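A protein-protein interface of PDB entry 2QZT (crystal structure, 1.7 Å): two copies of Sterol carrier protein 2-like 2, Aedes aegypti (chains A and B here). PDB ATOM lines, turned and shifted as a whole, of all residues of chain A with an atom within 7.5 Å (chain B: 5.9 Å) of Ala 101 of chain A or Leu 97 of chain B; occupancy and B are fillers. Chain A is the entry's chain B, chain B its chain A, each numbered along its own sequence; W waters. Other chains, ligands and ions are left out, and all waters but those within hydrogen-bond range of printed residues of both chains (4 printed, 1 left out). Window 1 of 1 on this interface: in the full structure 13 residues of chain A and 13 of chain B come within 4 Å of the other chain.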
ATOM      1  N   ASP A  66      -4.223 -14.902  14.726  1.00  0.00           N
ATOM      2  CA  ASP A  66      -4.945 -15.697  13.730  1.00  0.00           C
ATOM      3  C   ASP A  66      -6.115 -14.948  13.112  1.00  0.00           C
ATOM      4  O   ASP A  66      -6.403 -15.094  11.928  1.00  0.00           O
ATOM      5  CB  ASP A  66      -5.448 -16.980  14.370  1.00  0.00           C
ATOM      6  CG  ASP A  66      -4.323 -17.863  14.785  1.00  0.00           C
ATOM      7  OD1 ASP A  66      -3.692 -18.473  13.891  1.00  0.00           O
ATOM      8  OD2 ASP A  66      -4.054 -17.946  15.981  1.00  0.00           O
ATOM      9  N   VAL A  67      -6.787 -14.160  13.939  1.00  0.00           N
ATOM     10  CA  VAL A  67      -7.937 -13.347  13.509  1.00  0.00           C
ATOM     11  C   VAL A  67      -7.820 -12.018  14.219  1.00  0.00           C
ATOM     12  O   VAL A  67      -7.444 -11.968  15.408  1.00  0.00           O
ATOM     13  CB  VAL A  67      -9.304 -14.014  13.874  1.00  0.00           C
ATOM     14  CG1 VAL A  67     -10.518 -13.135  13.382  1.00  0.00           C
ATOM     15  CG2 VAL A  67      -9.410 -15.447  13.231  1.00  0.00           C
ATOM     16  N   LEU A  97     -13.266  -7.892  10.103  1.00  0.00           N
ATOM     17  CA  LEU A  97     -12.389  -9.044  10.378  1.00  0.00           C
ATOM     18  C   LEU A  97     -11.188  -8.994   9.466  1.00  0.00           C
ATOM     19  O   LEU A  97     -11.246  -8.431   8.360  1.00  0.00           O
ATOM     20  CB  LEU A  97     -13.098 -10.372  10.077  1.00  0.00           C
ATOM     21  CG  LEU A  97     -14.218 -10.770  10.996  1.00  0.00           C
ATOM     22  CD1 LEU A  97     -14.687 -12.151  10.577  1.00  0.00           C
ATOM     23  CD2 LEU A  97     -13.837 -10.752  12.502  1.00  0.00           C
ATOM     24  N   SER A  98     -10.086  -9.592   9.926  1.00  0.00           N
ATOM     25  CA  SER A  98      -8.990  -9.952   9.009  1.00  0.00           C
ATOM     26  C   SER A  98      -8.435 -11.265   9.547  1.00  0.00           C
ATOM     27  O   SER A  98      -8.706 -11.628  10.700  1.00  0.00           O
ATOM     28  CB  SER A  98      -7.919  -8.850   8.858  1.00  0.00           C
ATOM     29  OG  SER A  98      -7.207  -8.617  10.051  1.00  0.00           O
ATOM     30  N   GLY A  99      -7.765 -12.043   8.715  1.00  0.00           N
ATOM     31  CA  GLY A  99      -7.185 -13.272   9.215  1.00  0.00           C
ATOM     32  C   GLY A  99      -7.892 -14.511   8.757  1.00  0.00           C
ATOM     33  O   GLY A  99      -8.299 -14.597   7.594  1.00  0.00           O
ATOM     34  N   ASP A 100      -8.009 -15.483   9.656  1.00  0.00           N
ATOM     35  CA  ASP A 100      -8.381 -16.863   9.300  1.00  0.00           C
ATOM     36  C   ASP A 100      -9.894 -17.060   9.352  1.00  0.00           C
ATOM     37  O   ASP A 100     -10.482 -17.015  10.410  1.00  0.00           O
ATOM     38  CB  ASP A 100      -7.609 -17.820  10.247  1.00  0.00           C
ATOM     39  CG  ASP A 100      -7.927 -19.281  10.047  1.00  0.00           C
ATOM     40  OD1 ASP A 100      -7.167 -20.130  10.592  1.00  0.00           O
ATOM     41  OD2 ASP A 100      -8.898 -19.600   9.345  1.00  0.00           O
ATOM     42  N   ALA A 101     -10.523 -17.250   8.191  1.00  0.00           N
ATOM     43  CA  ALA A 101     -11.988 -17.353   8.139  1.00  0.00           C
ATOM     44  C   ALA A 101     -12.499 -18.592   8.860  1.00  0.00           C
ATOM     45  O   ALA A 101     -13.618 -18.589   9.398  1.00  0.00           O
ATOM     46  CB  ALA A 101     -12.455 -17.349   6.684  1.00  0.00           C
ATOM     47  N   ASP A 102     -11.730 -19.674   8.819  1.00  0.00           N
ATOM     48  CA  ASP A 102     -12.127 -20.896   9.539  1.00  0.00           C
ATOM     49  C   ASP A 102     -12.255 -20.621  11.044  1.00  0.00           C
ATOM     50  O   ASP A 102     -13.259 -20.944  11.679  1.00  0.00           O
ATOM     51  CB  ASP A 102     -11.095 -21.991   9.261  1.00  0.00           C
ATOM     52  CG  ASP A 102     -11.355 -23.235  10.030  1.00  0.00           C
ATOM     53  OD1 ASP A 102     -10.397 -23.717  10.669  1.00  0.00           O
ATOM     54  OD2 ASP A 102     -12.504 -23.724  10.034  1.00  0.00           O
ATOM     55  N   LEU A 103     -11.239 -20.004  11.618  1.00  0.00           N
ATOM     56  CA  LEU A 103     -11.319 -19.674  13.029  1.00  0.00           C
ATOM     57  C   LEU A 103     -12.415 -18.660  13.347  1.00  0.00           C
ATOM     58  O   LEU A 103     -13.024 -18.732  14.415  1.00  0.00           O
ATOM     59  CB  LEU A 103      -9.957 -19.189  13.526  1.00  0.00           C
ATOM     60  CG  LEU A 103      -9.048 -20.369  13.874  1.00  0.00           C
ATOM     61  CD1 LEU A 103      -7.588 -19.961  14.017  1.00  0.00           C
ATOM     62  CD2 LEU A 103      -9.504 -21.021  15.194  1.00  0.00           C
ATOM     63  N   ALA A 104     -12.632 -17.691  12.461  1.00  0.00           N
ATOM     64  CA  ALA A 104     -13.729 -16.750  12.667  1.00  0.00           C
ATOM     65  C   ALA A 104     -15.077 -17.474  12.735  1.00  0.00           C
ATOM     66  O   ALA A 104     -15.920 -17.178  13.579  1.00  0.00           O
ATOM     67  CB  ALA A 104     -13.739 -15.708  11.557  1.00  0.00           C
ATOM     68  N   ALA A 105     -15.272 -18.437  11.849  1.00  0.00           N
ATOM     69  CA  ALA A 105     -16.551 -19.143  11.777  1.00  0.00           C
ATOM     70  C   ALA A 105     -16.742 -20.039  12.994  1.00  0.00           C
ATOM     71  O   ALA A 105     -17.855 -20.133  13.551  1.00  0.00           O
ATOM     72  CB  ALA A 105     -16.653 -19.926  10.485  1.00  0.00           C
ATOM     73  N   LYS A 106     -15.647 -20.652  13.441  1.00  0.00           N
ATOM     74  CA  LYS A 106     -15.667 -21.495  14.631  1.00  0.00           C
ATOM     75  C   LYS A 106     -16.052 -20.632  15.842  1.00  0.00           C
ATOM     76  O   LYS A 106     -16.894 -21.032  16.658  1.00  0.00           O
ATOM     77  CB  LYS A 106     -14.316 -22.213  14.833  1.00  0.00           C
ATOM     78  CG  LYS A 106     -14.006 -23.336  13.751  1.00  0.00           C
ATOM     79  CD  LYS A 106     -12.492 -23.755  13.712  1.00  0.00           C
ATOM     80  CE  LYS A 106     -12.267 -25.184  13.198  1.00  0.00           C
ATOM     81  NZ  LYS A 106     -10.800 -25.489  12.851  1.00  0.00           N
ATOM     82  N   LEU A 107     -15.459 -19.439  15.935  1.00  0.00           N
ATOM     83  CA  LEU A 107     -15.776 -18.541  17.062  1.00  0.00           C
ATOM     84  C   LEU A 107     -17.272 -18.188  17.035  1.00  0.00           C
ATOM     85  O   LEU A 107     -17.946 -18.280  18.068  1.00  0.00           O
ATOM     86  CB  LEU A 107     -14.935 -17.271  17.005  1.00  0.00           C
ATOM     87  CG  LEU A 107     -15.173 -16.380  18.233  1.00  0.00           C
ATOM     88  CD1 LEU A 107     -14.988 -17.140  19.580  1.00  0.00           C
ATOM     89  CD2 LEU A 107     -14.266 -15.150  18.159  1.00  0.00           C
ATOM     90  N   VAL B  67     -11.623 -17.385  -0.515  1.00  0.00           N
ATOM     91  CA  VAL B  67     -12.413 -17.989   0.557  1.00  0.00           C
ATOM     92  C   VAL B  67     -13.005 -19.287   0.043  1.00  0.00           C
ATOM     93  O   VAL B  67     -13.366 -19.366  -1.131  1.00  0.00           O
ATOM     94  CB  VAL B  67     -13.586 -17.052   1.021  1.00  0.00           C
ATOM     95  CG1 VAL B  67     -14.426 -17.775   2.097  1.00  0.00           C
ATOM     96  CG2 VAL B  67     -13.010 -15.741   1.609  1.00  0.00           C
ATOM     97  N   THR B  68     -13.102 -20.310   0.889  1.00  0.00           N
ATOM     98  CA  THR B  68     -13.831 -21.525   0.488  1.00  0.00           C
ATOM     99  C   THR B  68     -15.028 -21.675   1.434  1.00  0.00           C
ATOM    100  O   THR B  68     -14.892 -21.534   2.667  1.00  0.00           O
ATOM    101  CB  THR B  68     -12.935 -22.760   0.589  1.00  0.00           C
ATOM    102  OG1 THR B  68     -11.812 -22.627  -0.323  1.00  0.00           O
ATOM    103  CG2 THR B  68     -13.741 -24.023   0.313  1.00  0.00           C
ATOM    104  N   VAL B  69     -16.196 -21.937   0.862  1.00  0.00           N
ATOM    105  CA  VAL B  69     -17.431 -22.038   1.621  1.00  0.00           C
ATOM    106  C   VAL B  69     -18.022 -23.425   1.380  1.00  0.00           C
ATOM    107  O   VAL B  69     -18.249 -23.783   0.242  1.00  0.00           O
ATOM    108  CB  VAL B  69     -18.416 -20.974   1.128  1.00  0.00           C
ATOM    109  CG1 VAL B  69     -19.766 -21.038   1.872  1.00  0.00           C
ATOM    110  CG2 VAL B  69     -17.795 -19.556   1.313  1.00  0.00           C
ATOM    111  N   THR B  70     -18.247 -24.189   2.446  1.00  0.00           N
ATOM    112  CA  THR B  70     -18.825 -25.514   2.324  1.00  0.00           C
ATOM    113  C   THR B  70     -20.110 -25.588   3.134  1.00  0.00           C
ATOM    114  O   THR B  70     -20.104 -25.327   4.331  1.00  0.00           O
ATOM    115  CB  THR B  70     -17.798 -26.574   2.794  1.00  0.00           C
ATOM    116  OG1 THR B  70     -16.623 -26.437   1.978  1.00  0.00           O
ATOM    117  CG2 THR B  70     -18.370 -27.961   2.604  1.00  0.00           C
ATOM    118  N   LEU B  90     -24.600 -19.878  11.111  1.00  0.00           N
ATOM    119  CA  LEU B  90     -23.275 -19.787  11.740  1.00  0.00           C
ATOM    120  C   LEU B  90     -23.301 -20.349  13.162  1.00  0.00           C
ATOM    121  O   LEU B  90     -22.454 -21.176  13.530  1.00  0.00           O
ATOM    122  CB  LEU B  90     -22.779 -18.333  11.747  1.00  0.00           C
ATOM    123  CG  LEU B  90     -22.295 -17.749  10.410  1.00  0.00           C
ATOM    124  CD1 LEU B  90     -22.090 -16.221  10.478  1.00  0.00           C
ATOM    125  CD2 LEU B  90     -21.003 -18.421   9.912  1.00  0.00           C
ATOM    126  N   ILE B  95     -22.021 -23.702   8.373  1.00  0.00           N
ATOM    127  CA  ILE B  95     -21.181 -23.139   7.316  1.00  0.00           C
ATOM    128  C   ILE B  95     -19.723 -23.332   7.661  1.00  0.00           C
ATOM    129  O   ILE B  95     -19.231 -22.843   8.683  1.00  0.00           O
ATOM    130  CB  ILE B  95     -21.432 -21.633   7.105  1.00  0.00           C
ATOM    131  CG1 ILE B  95     -22.896 -21.404   6.730  1.00  0.00           C
ATOM    132  CG2 ILE B  95     -20.528 -21.100   5.989  1.00  0.00           C
ATOM    133  CD1 ILE B  95     -23.322 -19.954   6.760  1.00  0.00           C
ATOM    134  N   GLU B  96     -19.022 -24.018   6.790  1.00  0.00           N
ATOM    135  CA  GLU B  96     -17.601 -24.262   6.995  1.00  0.00           C
ATOM    136  C   GLU B  96     -16.842 -23.343   6.076  1.00  0.00           C
ATOM    137  O   GLU B  96     -17.148 -23.271   4.875  1.00  0.00           O
ATOM    138  CB  GLU B  96     -17.274 -25.714   6.678  1.00  0.00           C
ATOM    139  CG  GLU B  96     -15.780 -26.053   6.685  1.00  0.00           C
ATOM    140  CD  GLU B  96     -15.515 -27.480   6.172  1.00  0.00           C
ATOM    141  OE1 GLU B  96     -14.546 -27.682   5.397  1.00  0.00           O
ATOM    142  OE2 GLU B  96     -16.293 -28.397   6.509  1.00  0.00           O
ATOM    143  N   LEU B  97     -15.865 -22.625   6.637  1.00  0.00           N
ATOM    144  CA  LEU B  97     -15.069 -21.672   5.851  1.00  0.00           C
ATOM    145  C   LEU B  97     -13.599 -22.008   5.925  1.00  0.00           C
ATOM    146  O   LEU B  97     -13.144 -22.607   6.908  1.00  0.00           O
ATOM    147  CB  LEU B  97     -15.210 -20.258   6.429  1.00  0.00           C
ATOM    148  CG  LEU B  97     -16.599 -19.652   6.502  1.00  0.00           C
ATOM    149  CD1 LEU B  97     -16.485 -18.237   7.084  1.00  0.00           C
ATOM    150  CD2 LEU B  97     -17.269 -19.661   5.105  1.00  0.00           C
ATOM    151  N   SER B  98     -12.868 -21.576   4.905  1.00  0.00           N
ATOM    152  CA  SER B  98     -11.422 -21.397   5.031  1.00  0.00           C
ATOM    153  C   SER B  98     -11.025 -20.157   4.247  1.00  0.00           C
ATOM    154  O   SER B  98     -11.792 -19.687   3.389  1.00  0.00           O
ATOM    155  CB  SER B  98     -10.624 -22.648   4.606  1.00  0.00           C
ATOM    156  OG  SER B  98     -10.766 -22.912   3.226  1.00  0.00           O
ATOM    157  N   GLY B  99      -9.869 -19.584   4.565  1.00  0.00           N
ATOM    158  CA  GLY B  99      -9.382 -18.491   3.761  1.00  0.00           C
ATOM    159  C   GLY B  99      -9.486 -17.191   4.500  1.00  0.00           C
ATOM    160  O   GLY B  99      -9.222 -17.143   5.686  1.00  0.00           O
ATOM    161  N   ASP B 100      -9.871 -16.151   3.767  1.00  0.00           N
ATOM    162  CA  ASP B 100      -9.746 -14.754   4.216  1.00  0.00           C
ATOM    163  C   ASP B 100     -10.979 -14.334   4.989  1.00  0.00           C
ATOM    164  O   ASP B 100     -12.076 -14.224   4.398  1.00  0.00           O
ATOM    165  CB  ASP B 100      -9.586 -13.905   2.968  1.00  0.00           C
ATOM    166  CG  ASP B 100      -9.374 -12.466   3.246  1.00  0.00           C
ATOM    167  OD1 ASP B 100      -8.976 -11.770   2.279  1.00  0.00           O
ATOM    168  OD2 ASP B 100      -9.519 -12.012   4.400  1.00  0.00           O
ATOM    169  N   ALA B 101     -10.800 -14.077   6.292  1.00  0.00           N
ATOM    170  CA  ALA B 101     -11.923 -13.681   7.131  1.00  0.00           C
ATOM    171  C   ALA B 101     -12.526 -12.333   6.720  1.00  0.00           C
ATOM    172  O   ALA B 101     -13.731 -12.102   6.877  1.00  0.00           O
ATOM    173  CB  ALA B 101     -11.502 -13.654   8.616  1.00  0.00           C
ATOM    174  N   ALA B 104     -14.819 -13.037   3.715  1.00  0.00           N
ATOM    175  CA  ALA B 104     -16.008 -13.767   4.195  1.00  0.00           C
ATOM    176  C   ALA B 104     -16.979 -12.824   4.935  1.00  0.00           C
ATOM    177  O   ALA B 104     -18.218 -12.924   4.816  1.00  0.00           O
ATOM    178  CB  ALA B 104     -15.585 -14.849   5.117  1.00  0.00           C
HETATM  179  O   HOH W   1      -6.299 -16.126   5.620  1.00  0.00           O
HETATM  180  O   HOH W   2      -8.671 -20.748   6.910  1.00  0.00           O
HETATM  181  O   HOH W   3      -7.761 -10.977   6.001  1.00  0.00           O
HETATM  182  O   HOH W   4     -15.089 -23.129   9.332  1.00  0.00           O
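Ala 101 of chain B touches Leu 97 of chain A (O to CB, 3.7 Å). Ser 98 of chain A touches Ala 101 of chain B. O of Gly 99 of chain A touches CA of Asp 100 of chain B (3.7 Å). Asp 100 of chain A touches Gly 99 of chain B. C of Asp 100 of chain A touches CB of Ala 101 of chain B (3.8 Å). O of Ala 101 of chain A touches CD1 of Leu 97 of chain B, 3.7 Å away. Ser 98 of chain B touches Ala 101 of chain A (C to CB, 3.98 Å). Asp 100 of chain B touches Ala 101 of chain A. CB of Ala 101 of chain A touches N of Ala 101 of chain B (3.7 Å). Leu 97 of chain B touches Ala 105 of chain A.
N of Ala 101 of chain A lies within hydrogen-bond range of O of Gly 99 of chain B. The backbone carbonyl oxygen (O) of Gly 99 of chain A sits at hydrogen-bond distance from the backbone NH (N) of Ala 101 of chain B (2.9 Å). The backbone carbonyl oxygen (O) of Gly 99 of chain A sits close to the backbone carbonyl oxygen (O) of Gly 99 of chain B (3.3 Å). The side-chain carboxylate of Asp 102 of chain A lies close to the backbone carbonyl oxygen of Leu 97 of chain B (3.4 Å).
Of the 13 printed residues of chain B, 5 touch a printed residue of chain A. Hydrophobic or aromatic side chains of chain B within 4 Å of the printed part of chain A: Leu 97 and Ala 101. Of the 13 printed residues of chain A, 7 touch a printed residue of chain B. Among the printed residues, 14 pairs touch across the chains.
Leu 97 of chain A touches Ala 101 of chain B, and with the chains exchanged Ala 101 of chain A touches Leu 97 of chain B. Ser 98 of chain A touches Ala 101 of chain B, and with the chains exchanged Ala 101 of chain A touches Ser 98 of chain B. Gly 99 of chain A touches Ala 101 of chain B, and with the chains exchanged Ala 101 of chain A touches Gly 99 of chain B. Ala 101 of chain B touches its own counterpart, Ala 101 of chain A. Positions printed for both chains: 67, 97, 98, 99, 100, 101 and 104. Of the 14 pairs that touch across the chains among the printed residues, 12 have their exchanged pair printed and touching as well.
Of the printed residues of chain B, Ala 101 of chain A touches Leu 97, Ser 98, Gly 99, Asp 100 and Ala 101. Of chain A, only Ala 101, Asp 102 and Ala 105 come within 4 Å of Leu 97 of chain B. Of the printed residues of chain A, Ala 101 of chain B touches Leu 97 (3.7 Å), Ser 98 (3.998 Å), Gly 99 (2.9 Å), Asp 100 (3.8 Å) and Ala 101 (3.7 Å). Printed residues of chain A within 4 Å of Asp 100 of chain B: Gly 99 and Ala 101. Printed residues of chain B within 4 Å of Ala 105 of chain A: Leu 97 (3.8 Å). Printed residues of chain B within 4 Å of Asp 100 of chain A: Gly 99 and Ala 101. Printed residues of chain B within 4 Å of Ser 98 of chain A: Ala 101 (3.998 Å). The nearest printed residue of chain B that does not touch Ala 101 of chain A is Ala 104 of chain B (4.3 Å). The nearest residue of chain A that does not touch Leu 97 of chain B is Leu 103 of chain A (5.7 Å). The nearest printed residue of chain B that does not touch Asp 100 of chain A is Asp 100 of chain B (5.3 Å).
Water W3 bridges OD2 of Asp 100 of chain B (2.6 Å) and N of Gly 99 of chain A (2.9 Å). Water W2 lies within hydrogen-bond range of OD2 of Asp 100 of chain A (2.7 Å) and N of Gly 99 of chain B (2.9 Å). Water W4 bridges OD2 of Asp 102 of chain A (2.7 Å) and N of Leu 97 of chain B (2.8 Å). Water W1 bridges O of Gly 99 of chain B (3.1 Å) and O of Gly 99 of chain A (3.2 Å).
N of Thr 68 of chain B is in hydrogen-bond range of O of Ser 98 of chain B, 2.9 Å away. The backbone carbonyl oxygen (O) of Asp 66 of chain A lies within hydrogen-bond range of the backbone NH (N) of Asp 100 of chain A (2.8 Å). N of Asp 102 of chain A lies within hydrogen-bond range of OD2 of Asp 100 of chain A. The side-chain carboxylate (OD2) of Asp 100 of chain A is in hydrogen-bond range of the backbone NH (N) of Leu 103 of chain A, 3.3 Å away. NZ of Lys 106 of chain A is in salt-bridge range of OD1 of Asp 102 of chain A (2.8 Å).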
